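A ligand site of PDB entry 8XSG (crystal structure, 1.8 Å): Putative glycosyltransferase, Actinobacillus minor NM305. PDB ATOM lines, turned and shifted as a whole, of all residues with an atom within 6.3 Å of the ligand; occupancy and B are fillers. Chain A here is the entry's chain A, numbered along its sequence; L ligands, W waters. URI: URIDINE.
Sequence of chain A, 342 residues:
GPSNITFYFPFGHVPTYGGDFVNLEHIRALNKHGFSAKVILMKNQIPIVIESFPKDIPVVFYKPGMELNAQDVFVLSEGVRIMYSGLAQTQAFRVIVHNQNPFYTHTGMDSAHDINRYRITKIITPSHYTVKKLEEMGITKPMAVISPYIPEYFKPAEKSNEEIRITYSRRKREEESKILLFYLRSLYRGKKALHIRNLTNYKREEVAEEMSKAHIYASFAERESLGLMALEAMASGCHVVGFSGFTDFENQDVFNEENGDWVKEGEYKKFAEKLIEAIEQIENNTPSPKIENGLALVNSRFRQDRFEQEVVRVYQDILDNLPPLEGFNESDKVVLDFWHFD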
ATOM      1  N   TYR A  17     -14.092  26.740  21.516  1.00  0.00           N
ATOM      2  CA  TYR A  17     -13.494  27.017  20.227  1.00  0.00           C
ATOM      3  C   TYR A  17     -12.555  28.177  20.473  1.00  0.00           C
ATOM      4  O   TYR A  17     -12.686  28.823  21.513  1.00  0.00           O
ATOM      5  CB  TYR A  17     -14.571  27.321  19.183  1.00  0.00           C
ATOM      6  CG  TYR A  17     -15.645  26.275  19.095  1.00  0.00           C
ATOM      7  CD1 TYR A  17     -15.391  25.052  18.496  1.00  0.00           C
ATOM      8  CD2 TYR A  17     -16.906  26.504  19.625  1.00  0.00           C
ATOM      9  CE1 TYR A  17     -16.365  24.067  18.415  1.00  0.00           C
ATOM     10  CE2 TYR A  17     -17.895  25.532  19.559  1.00  0.00           C
ATOM     11  CZ  TYR A  17     -17.625  24.325  18.940  1.00  0.00           C
ATOM     12  OH  TYR A  17     -18.577  23.339  18.859  1.00  0.00           O
ATOM     13  N   GLY A  18     -11.642  28.413  19.525  1.00  0.00           N
ATOM     14  CA  GLY A  18     -10.725  29.526  19.654  1.00  0.00           C
ATOM     15  C   GLY A  18     -11.505  30.822  19.916  1.00  0.00           C
ATOM     16  O   GLY A  18     -11.127  31.571  20.810  1.00  0.00           O
ATOM     17  N   PHE A 154       3.764  30.654  24.381  1.00  0.00           N
ATOM     18  CA  PHE A 154       4.273  30.181  23.108  1.00  0.00           C
ATOM     19  C   PHE A 154       5.558  30.921  22.800  1.00  0.00           C
ATOM     20  O   PHE A 154       5.538  32.128  22.524  1.00  0.00           O
ATOM     21  CB  PHE A 154       3.308  30.403  21.930  1.00  0.00           C
ATOM     22  CG  PHE A 154       2.078  29.536  21.919  1.00  0.00           C
ATOM     23  CD1 PHE A 154       0.919  29.955  22.550  1.00  0.00           C
ATOM     24  CD2 PHE A 154       2.052  28.338  21.219  1.00  0.00           C
ATOM     25  CE1 PHE A 154      -0.223  29.178  22.543  1.00  0.00           C
ATOM     26  CE2 PHE A 154       0.906  27.569  21.202  1.00  0.00           C
ATOM     27  CZ  PHE A 154      -0.232  27.981  21.857  1.00  0.00           C
ATOM     28  N   SER A 169      -2.002  19.166  12.960  1.00  0.00           N
ATOM     29  CA  SER A 169      -3.307  18.975  13.559  1.00  0.00           C
ATOM     30  C   SER A 169      -4.263  18.332  12.571  1.00  0.00           C
ATOM     31  O   SER A 169      -4.273  18.700  11.394  1.00  0.00           O
ATOM     32  CB  SER A 169      -3.868  20.272  14.077  1.00  0.00           C
ATOM     33  OG  SER A 169      -5.171  20.116  14.602  1.00  0.00           O
ATOM     34  N   ARG A 171      -7.552  18.758  13.160  1.00  0.00           N
ATOM     35  CA  ARG A 171      -8.788  19.520  13.370  1.00  0.00           C
ATOM     36  C   ARG A 171      -9.420  19.864  12.019  1.00  0.00           C
ATOM     37  O   ARG A 171     -10.638  19.820  11.888  1.00  0.00           O
ATOM     38  CB  ARG A 171      -8.546  20.807  14.172  1.00  0.00           C
ATOM     39  CG  ARG A 171      -9.828  21.581  14.492  1.00  0.00           C
ATOM     40  CD  ARG A 171      -9.751  22.501  15.722  1.00  0.00           C
ATOM     41  NE  ARG A 171      -8.718  23.527  15.581  1.00  0.00           N
ATOM     42  CZ  ARG A 171      -8.923  24.759  15.097  1.00  0.00           C
ATOM     43  NH1 ARG A 171     -10.084  25.371  15.254  1.00  0.00           N
ATOM     44  NH2 ARG A 171      -7.912  25.406  14.534  1.00  0.00           N
ATOM     45  N   LYS A 172      -8.608  20.197  11.014  1.00  0.00           N
ATOM     46  CA  LYS A 172      -9.151  20.471   9.688  1.00  0.00           C
ATOM     47  C   LYS A 172      -8.419  19.575   8.683  1.00  0.00           C
ATOM     48  O   LYS A 172      -7.267  19.238   8.884  1.00  0.00           O
ATOM     49  CB  LYS A 172      -8.935  21.951   9.336  1.00  0.00           C
ATOM     50  CG  LYS A 172      -9.583  22.891  10.320  1.00  0.00           C
ATOM     51  CD  LYS A 172      -9.390  24.336  10.043  1.00  0.00           C
ATOM     52  CE  LYS A 172     -10.122  25.195  11.046  1.00  0.00           C
ATOM     53  NZ  LYS A 172     -10.205  26.593  10.551  1.00  0.00           N
ATOM     54  N   LEU A 199      -1.341  17.124  17.209  1.00  0.00           N
ATOM     55  CA  LEU A 199      -1.868  18.006  18.236  1.00  0.00           C
ATOM     56  C   LEU A 199      -3.347  18.205  17.959  1.00  0.00           C
ATOM     57  O   LEU A 199      -3.696  19.162  17.272  1.00  0.00           O
ATOM     58  CB  LEU A 199      -1.145  19.349  18.110  1.00  0.00           C
ATOM     59  CG  LEU A 199       0.385  19.290  18.059  1.00  0.00           C
ATOM     60  CD1 LEU A 199       0.975  20.682  17.934  1.00  0.00           C
ATOM     61  CD2 LEU A 199       0.974  18.612  19.296  1.00  0.00           C
ATOM     62  N   THR A 200      -4.230  17.288  18.334  1.00  0.00           N
ATOM     63  CA  THR A 200      -5.645  17.531  18.052  1.00  0.00           C
ATOM     64  C   THR A 200      -6.433  17.664  19.342  1.00  0.00           C
ATOM     65  O   THR A 200      -7.194  18.619  19.500  1.00  0.00           O
ATOM     66  CB  THR A 200      -6.275  16.534  17.062  1.00  0.00           C
ATOM     67  OG1 THR A 200      -5.610  16.734  15.821  1.00  0.00           O
ATOM     68  CG2 THR A 200      -7.757  16.758  16.834  1.00  0.00           C
ATOM     69  N   ASN A 201      -6.318  16.747  20.292  1.00  0.00           N
ATOM     70  CA  ASN A 201      -7.213  17.013  21.415  1.00  0.00           C
ATOM     71  C   ASN A 201      -6.395  17.471  22.611  1.00  0.00           C
ATOM     72  O   ASN A 201      -6.564  16.956  23.711  1.00  0.00           O
ATOM     73  CB  ASN A 201      -8.192  15.856  21.639  1.00  0.00           C
ATOM     74  CG  ASN A 201      -9.210  15.730  20.507  1.00  0.00           C
ATOM     75  OD1 ASN A 201      -9.219  14.743  19.785  1.00  0.00           O
ATOM     76  ND2 ASN A 201     -10.057  16.746  20.320  1.00  0.00           N
ATOM     77  N   TYR A 202      -5.565  18.510  22.418  1.00  0.00           N
ATOM     78  CA  TYR A 202      -4.697  19.029  23.477  1.00  0.00           C
ATOM     79  C   TYR A 202      -5.217  20.363  23.983  1.00  0.00           C
ATOM     80  O   TYR A 202      -5.884  21.105  23.267  1.00  0.00           O
ATOM     81  CB  TYR A 202      -3.251  19.239  22.985  1.00  0.00           C
ATOM     82  CG  TYR A 202      -2.422  17.993  22.757  1.00  0.00           C
ATOM     83  CD1 TYR A 202      -2.795  16.987  21.878  1.00  0.00           C
ATOM     84  CD2 TYR A 202      -1.191  17.856  23.394  1.00  0.00           C
ATOM     85  CE1 TYR A 202      -1.987  15.877  21.673  1.00  0.00           C
ATOM     86  CE2 TYR A 202      -0.382  16.755  23.195  1.00  0.00           C
ATOM     87  CZ  TYR A 202      -0.778  15.764  22.328  1.00  0.00           C
ATOM     88  OH  TYR A 202       0.042  14.690  22.176  1.00  0.00           O
ATOM     89  N   LYS A 203      -4.870  20.717  25.216  1.00  0.00           N
ATOM     90  CA  LYS A 203      -5.186  22.022  25.762  1.00  0.00           C
ATOM     91  C   LYS A 203      -4.144  22.989  25.203  1.00  0.00           C
ATOM     92  O   LYS A 203      -3.075  22.563  24.785  1.00  0.00           O
ATOM     93  CB  LYS A 203      -5.177  22.018  27.300  1.00  0.00           C
ATOM     94  CG  LYS A 203      -5.779  20.817  28.028  1.00  0.00           C
ATOM     95  CD  LYS A 203      -6.940  20.060  27.347  1.00  0.00           C
ATOM     96  CE  LYS A 203      -8.163  20.904  27.063  1.00  0.00           C
ATOM     97  NZ  LYS A 203      -8.877  21.302  28.298  1.00  0.00           N
ATOM     98  N   ARG A 204      -4.444  24.284  25.225  1.00  0.00           N
ATOM     99  CA  ARG A 204      -3.618  25.237  24.521  1.00  0.00           C
ATOM    100  C   ARG A 204      -2.211  25.290  25.103  1.00  0.00           C
ATOM    101  O   ARG A 204      -1.254  25.394  24.334  1.00  0.00           O
ATOM    102  CB  ARG A 204      -4.260  26.626  24.483  1.00  0.00           C
ATOM    103  CG  ARG A 204      -3.743  27.432  23.303  1.00  0.00           C
ATOM    104  CD  ARG A 204      -4.322  28.814  23.322  1.00  0.00           C
ATOM    105  NE  ARG A 204      -3.875  29.557  22.171  1.00  0.00           N
ATOM    106  CZ  ARG A 204      -4.150  30.845  22.011  1.00  0.00           C
ATOM    107  NH1 ARG A 204      -4.832  31.465  22.944  1.00  0.00           N
ATOM    108  NH2 ARG A 204      -3.720  31.499  20.954  1.00  0.00           N
ATOM    109  N   GLU A 205      -2.059  25.205  26.442  1.00  0.00           N
ATOM    110  CA  GLU A 205      -0.746  25.219  27.071  1.00  0.00           C
ATOM    111  C   GLU A 205       0.080  24.014  26.604  1.00  0.00           C
ATOM    112  O   GLU A 205       1.296  24.098  26.465  1.00  0.00           O
ATOM    113  CB  GLU A 205      -0.822  25.201  28.608  1.00  0.00           C
ATOM    114  CG  GLU A 205      -1.340  26.492  29.230  1.00  0.00           C
ATOM    115  CD  GLU A 205      -2.850  26.661  29.146  1.00  0.00           C
ATOM    116  OE1 GLU A 205      -3.520  25.793  28.519  1.00  0.00           O
ATOM    117  OE2 GLU A 205      -3.358  27.668  29.674  1.00  0.00           O
ATOM    118  N   VAL A 207      -0.373  22.408  23.645  1.00  0.00           N
ATOM    119  CA  VAL A 207       0.034  22.723  22.274  1.00  0.00           C
ATOM    120  C   VAL A 207       1.367  23.483  22.306  1.00  0.00           C
ATOM    121  O   VAL A 207       2.270  23.223  21.523  1.00  0.00           O
ATOM    122  CB  VAL A 207      -1.032  23.519  21.513  1.00  0.00           C
ATOM    123  CG1 VAL A 207      -0.555  23.921  20.132  1.00  0.00           C
ATOM    124  CG2 VAL A 207      -2.311  22.743  21.375  1.00  0.00           C
ATOM    125  N   ALA A 208       1.438  24.510  23.153  1.00  0.00           N
ATOM    126  CA  ALA A 208       2.619  25.351  23.226  1.00  0.00           C
ATOM    127  C   ALA A 208       3.863  24.532  23.607  1.00  0.00           C
ATOM    128  O   ALA A 208       4.925  24.692  23.009  1.00  0.00           O
ATOM    129  CB  ALA A 208       2.344  26.485  24.203  1.00  0.00           C
ATOM    130  N   MET A 211       4.924  22.439  20.503  1.00  0.00           N
ATOM    131  CA  MET A 211       5.476  23.274  19.447  1.00  0.00           C
ATOM    132  C   MET A 211       6.849  23.787  19.830  1.00  0.00           C
ATOM    133  O   MET A 211       7.731  23.879  18.964  1.00  0.00           O
ATOM    134  CB  MET A 211       4.579  24.463  19.126  1.00  0.00           C
ATOM    135  CG  MET A 211       3.345  24.070  18.332  1.00  0.00           C
ATOM    136  SD  MET A 211       2.404  25.524  17.986  1.00  0.00           S
ATOM    137  CE  MET A 211       1.061  24.850  17.011  1.00  0.00           C
ATOM    138  N   GLU A 224      -9.379  30.011   7.006  1.00  0.00           N
ATOM    139  CA  GLU A 224      -9.035  30.802   8.180  1.00  0.00           C
ATOM    140  C   GLU A 224      -9.393  32.294   8.006  1.00  0.00           C
ATOM    141  O   GLU A 224      -9.546  32.836   6.897  1.00  0.00           O
ATOM    142  CB  GLU A 224      -7.533  30.707   8.440  1.00  0.00           C
ATOM    143  CG  GLU A 224      -6.991  29.297   8.581  1.00  0.00           C
ATOM    144  CD  GLU A 224      -7.535  28.500   9.748  1.00  0.00           C
ATOM    145  OE1 GLU A 224      -7.971  29.144  10.721  1.00  0.00           O
ATOM    146  OE2 GLU A 224      -7.580  27.218   9.656  1.00  0.00           O
ATOM    147  N   LEU A 228      -4.328  31.096  13.628  1.00  0.00           N
ATOM    148  CA  LEU A 228      -3.740  31.017  14.955  1.00  0.00           C
ATOM    149  C   LEU A 228      -2.691  29.925  15.097  1.00  0.00           C
ATOM    150  O   LEU A 228      -1.672  30.145  15.720  1.00  0.00           O
ATOM    151  CB  LEU A 228      -4.842  30.776  15.983  1.00  0.00           C
ATOM    152  CG  LEU A 228      -5.505  32.036  16.544  1.00  0.00           C
ATOM    153  CD1 LEU A 228      -6.308  32.782  15.472  1.00  0.00           C
ATOM    154  CD2 LEU A 228      -6.395  31.676  17.722  1.00  0.00           C
ATOM    155  N   MET A 229      -2.949  28.712  14.615  1.00  0.00           N
ATOM    156  CA  MET A 229      -1.996  27.644  14.884  1.00  0.00           C
ATOM    157  C   MET A 229      -0.690  27.891  14.122  1.00  0.00           C
ATOM    158  O   MET A 229       0.377  27.586  14.660  1.00  0.00           O
ATOM    159  CB  MET A 229      -2.591  26.273  14.557  1.00  0.00           C
ATOM    160  CG  MET A 229      -3.476  25.721  15.701  1.00  0.00           C
ATOM    161  SD  MET A 229      -3.854  23.978  15.470  1.00  0.00           S
ATOM    162  CE  MET A 229      -2.479  23.191  16.322  1.00  0.00           C
ATOM    163  N   GLU A 232       1.090  30.444  16.238  1.00  0.00           N
ATOM    164  CA  GLU A 232       1.597  29.750  17.414  1.00  0.00           C
ATOM    165  C   GLU A 232       2.894  29.016  17.092  1.00  0.00           C
ATOM    166  O   GLU A 232       3.869  29.059  17.851  1.00  0.00           O
ATOM    167  CB  GLU A 232       0.528  28.776  17.901  1.00  0.00           C
ATOM    168  CG  GLU A 232      -0.639  29.479  18.595  1.00  0.00           C
ATOM    169  CD  GLU A 232      -1.828  28.606  18.941  1.00  0.00           C
ATOM    170  OE1 GLU A 232      -1.774  27.418  18.656  1.00  0.00           O
ATOM    171  OE2 GLU A 232      -2.779  29.120  19.523  1.00  0.00           O
HETATM  172  N1  URI L   1      -5.689  23.995  19.753  1.00  0.00           N
HETATM  173  C2  URI L   1      -5.689  23.528  21.051  1.00  0.00           C
HETATM  174  N3  URI L   1      -5.438  22.202  21.161  1.00  0.00           N
HETATM  175  C4  URI L   1      -5.137  21.306  20.162  1.00  0.00           C
HETATM  176  C5  URI L   1      -5.080  21.872  18.840  1.00  0.00           C
HETATM  177  C6  URI L   1      -5.369  23.173  18.695  1.00  0.00           C
HETATM  178  O2  URI L   1      -5.909  24.235  22.029  1.00  0.00           O
HETATM  179  O4  URI L   1      -4.939  20.140  20.486  1.00  0.00           O
HETATM  180  C1' URI L   1      -5.910  25.451  19.579  1.00  0.00           C
HETATM  181  C2' URI L   1      -4.665  26.132  19.011  1.00  0.00           C
HETATM  182  C3' URI L   1      -5.291  27.436  18.492  1.00  0.00           C
HETATM  183  C4' URI L   1      -6.746  27.043  18.103  1.00  0.00           C
HETATM  184  O2' URI L   1      -3.713  26.236  20.043  1.00  0.00           O
HETATM  185  O3' URI L   1      -5.267  28.454  19.508  1.00  0.00           O
HETATM  186  O4' URI L   1      -6.923  25.696  18.624  1.00  0.00           O
HETATM  187  C5' URI L   1      -7.033  27.083  16.594  1.00  0.00           C
HETATM  188  O5' URI L   1      -8.422  27.210  16.266  1.00  0.00           O
HETATM  189  O   HOH W   1      -7.199  29.443  21.336  1.00  0.00           O
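Water W1 lies within hydrogen-bond range of O3' of the ligand (2.8 Å) and NE of Arg 204 (3.4 Å).
O of Thr 200 lies close to O4 of the ligand.
Residues that only touch the ligand: Val 207 (3.2 Å), Leu 199 (3.4 Å), Met 229 (3.5 Å), Asn 201 (3.7 Å), Lys 203 (3.8 Å) and Leu 228 (3.9 Å).
Hydrophobic or aromatic side chains within 4 Å of the ligand: Tyr 202, Val 207, Leu 228 and Met 229.
Within 4 Å of the ligand: Arg 171, Leu 199, Thr 200, Asn 201, Tyr 202, Lys 203, Arg 204, Val 207, Leu 228, Met 229 and Glu 232.
N of Arg 171 sits at hydrogen-bond distance from OG of Ser 169.
NE of Arg 204 lies within salt-bridge range of OE2 of Glu 232 (2.9 Å).
OG of Ser 169 lies within hydrogen-bond range of O of Leu 199.
The backbone NH of Tyr 202 is in hydrogen-bond range of an oxygen (O4) of the ligand, 2.6 Å away.
The backbone carbonyl oxygen of Tyr 202 is in hydrogen-bond range of a nitrogen (N3) of the ligand, at 2.4 Å.
NH2 of Arg 171 sits at hydrogen-bond distance from O5' of the ligand.
An oxygen (O3') of the ligand lies within hydrogen-bond range of the side-chain carboxylate (OE2) of Glu 232.
The guanidinium group (NE) of Arg 204 lies within hydrogen-bond range of an oxygen (O3') of the ligand (3.2 Å).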
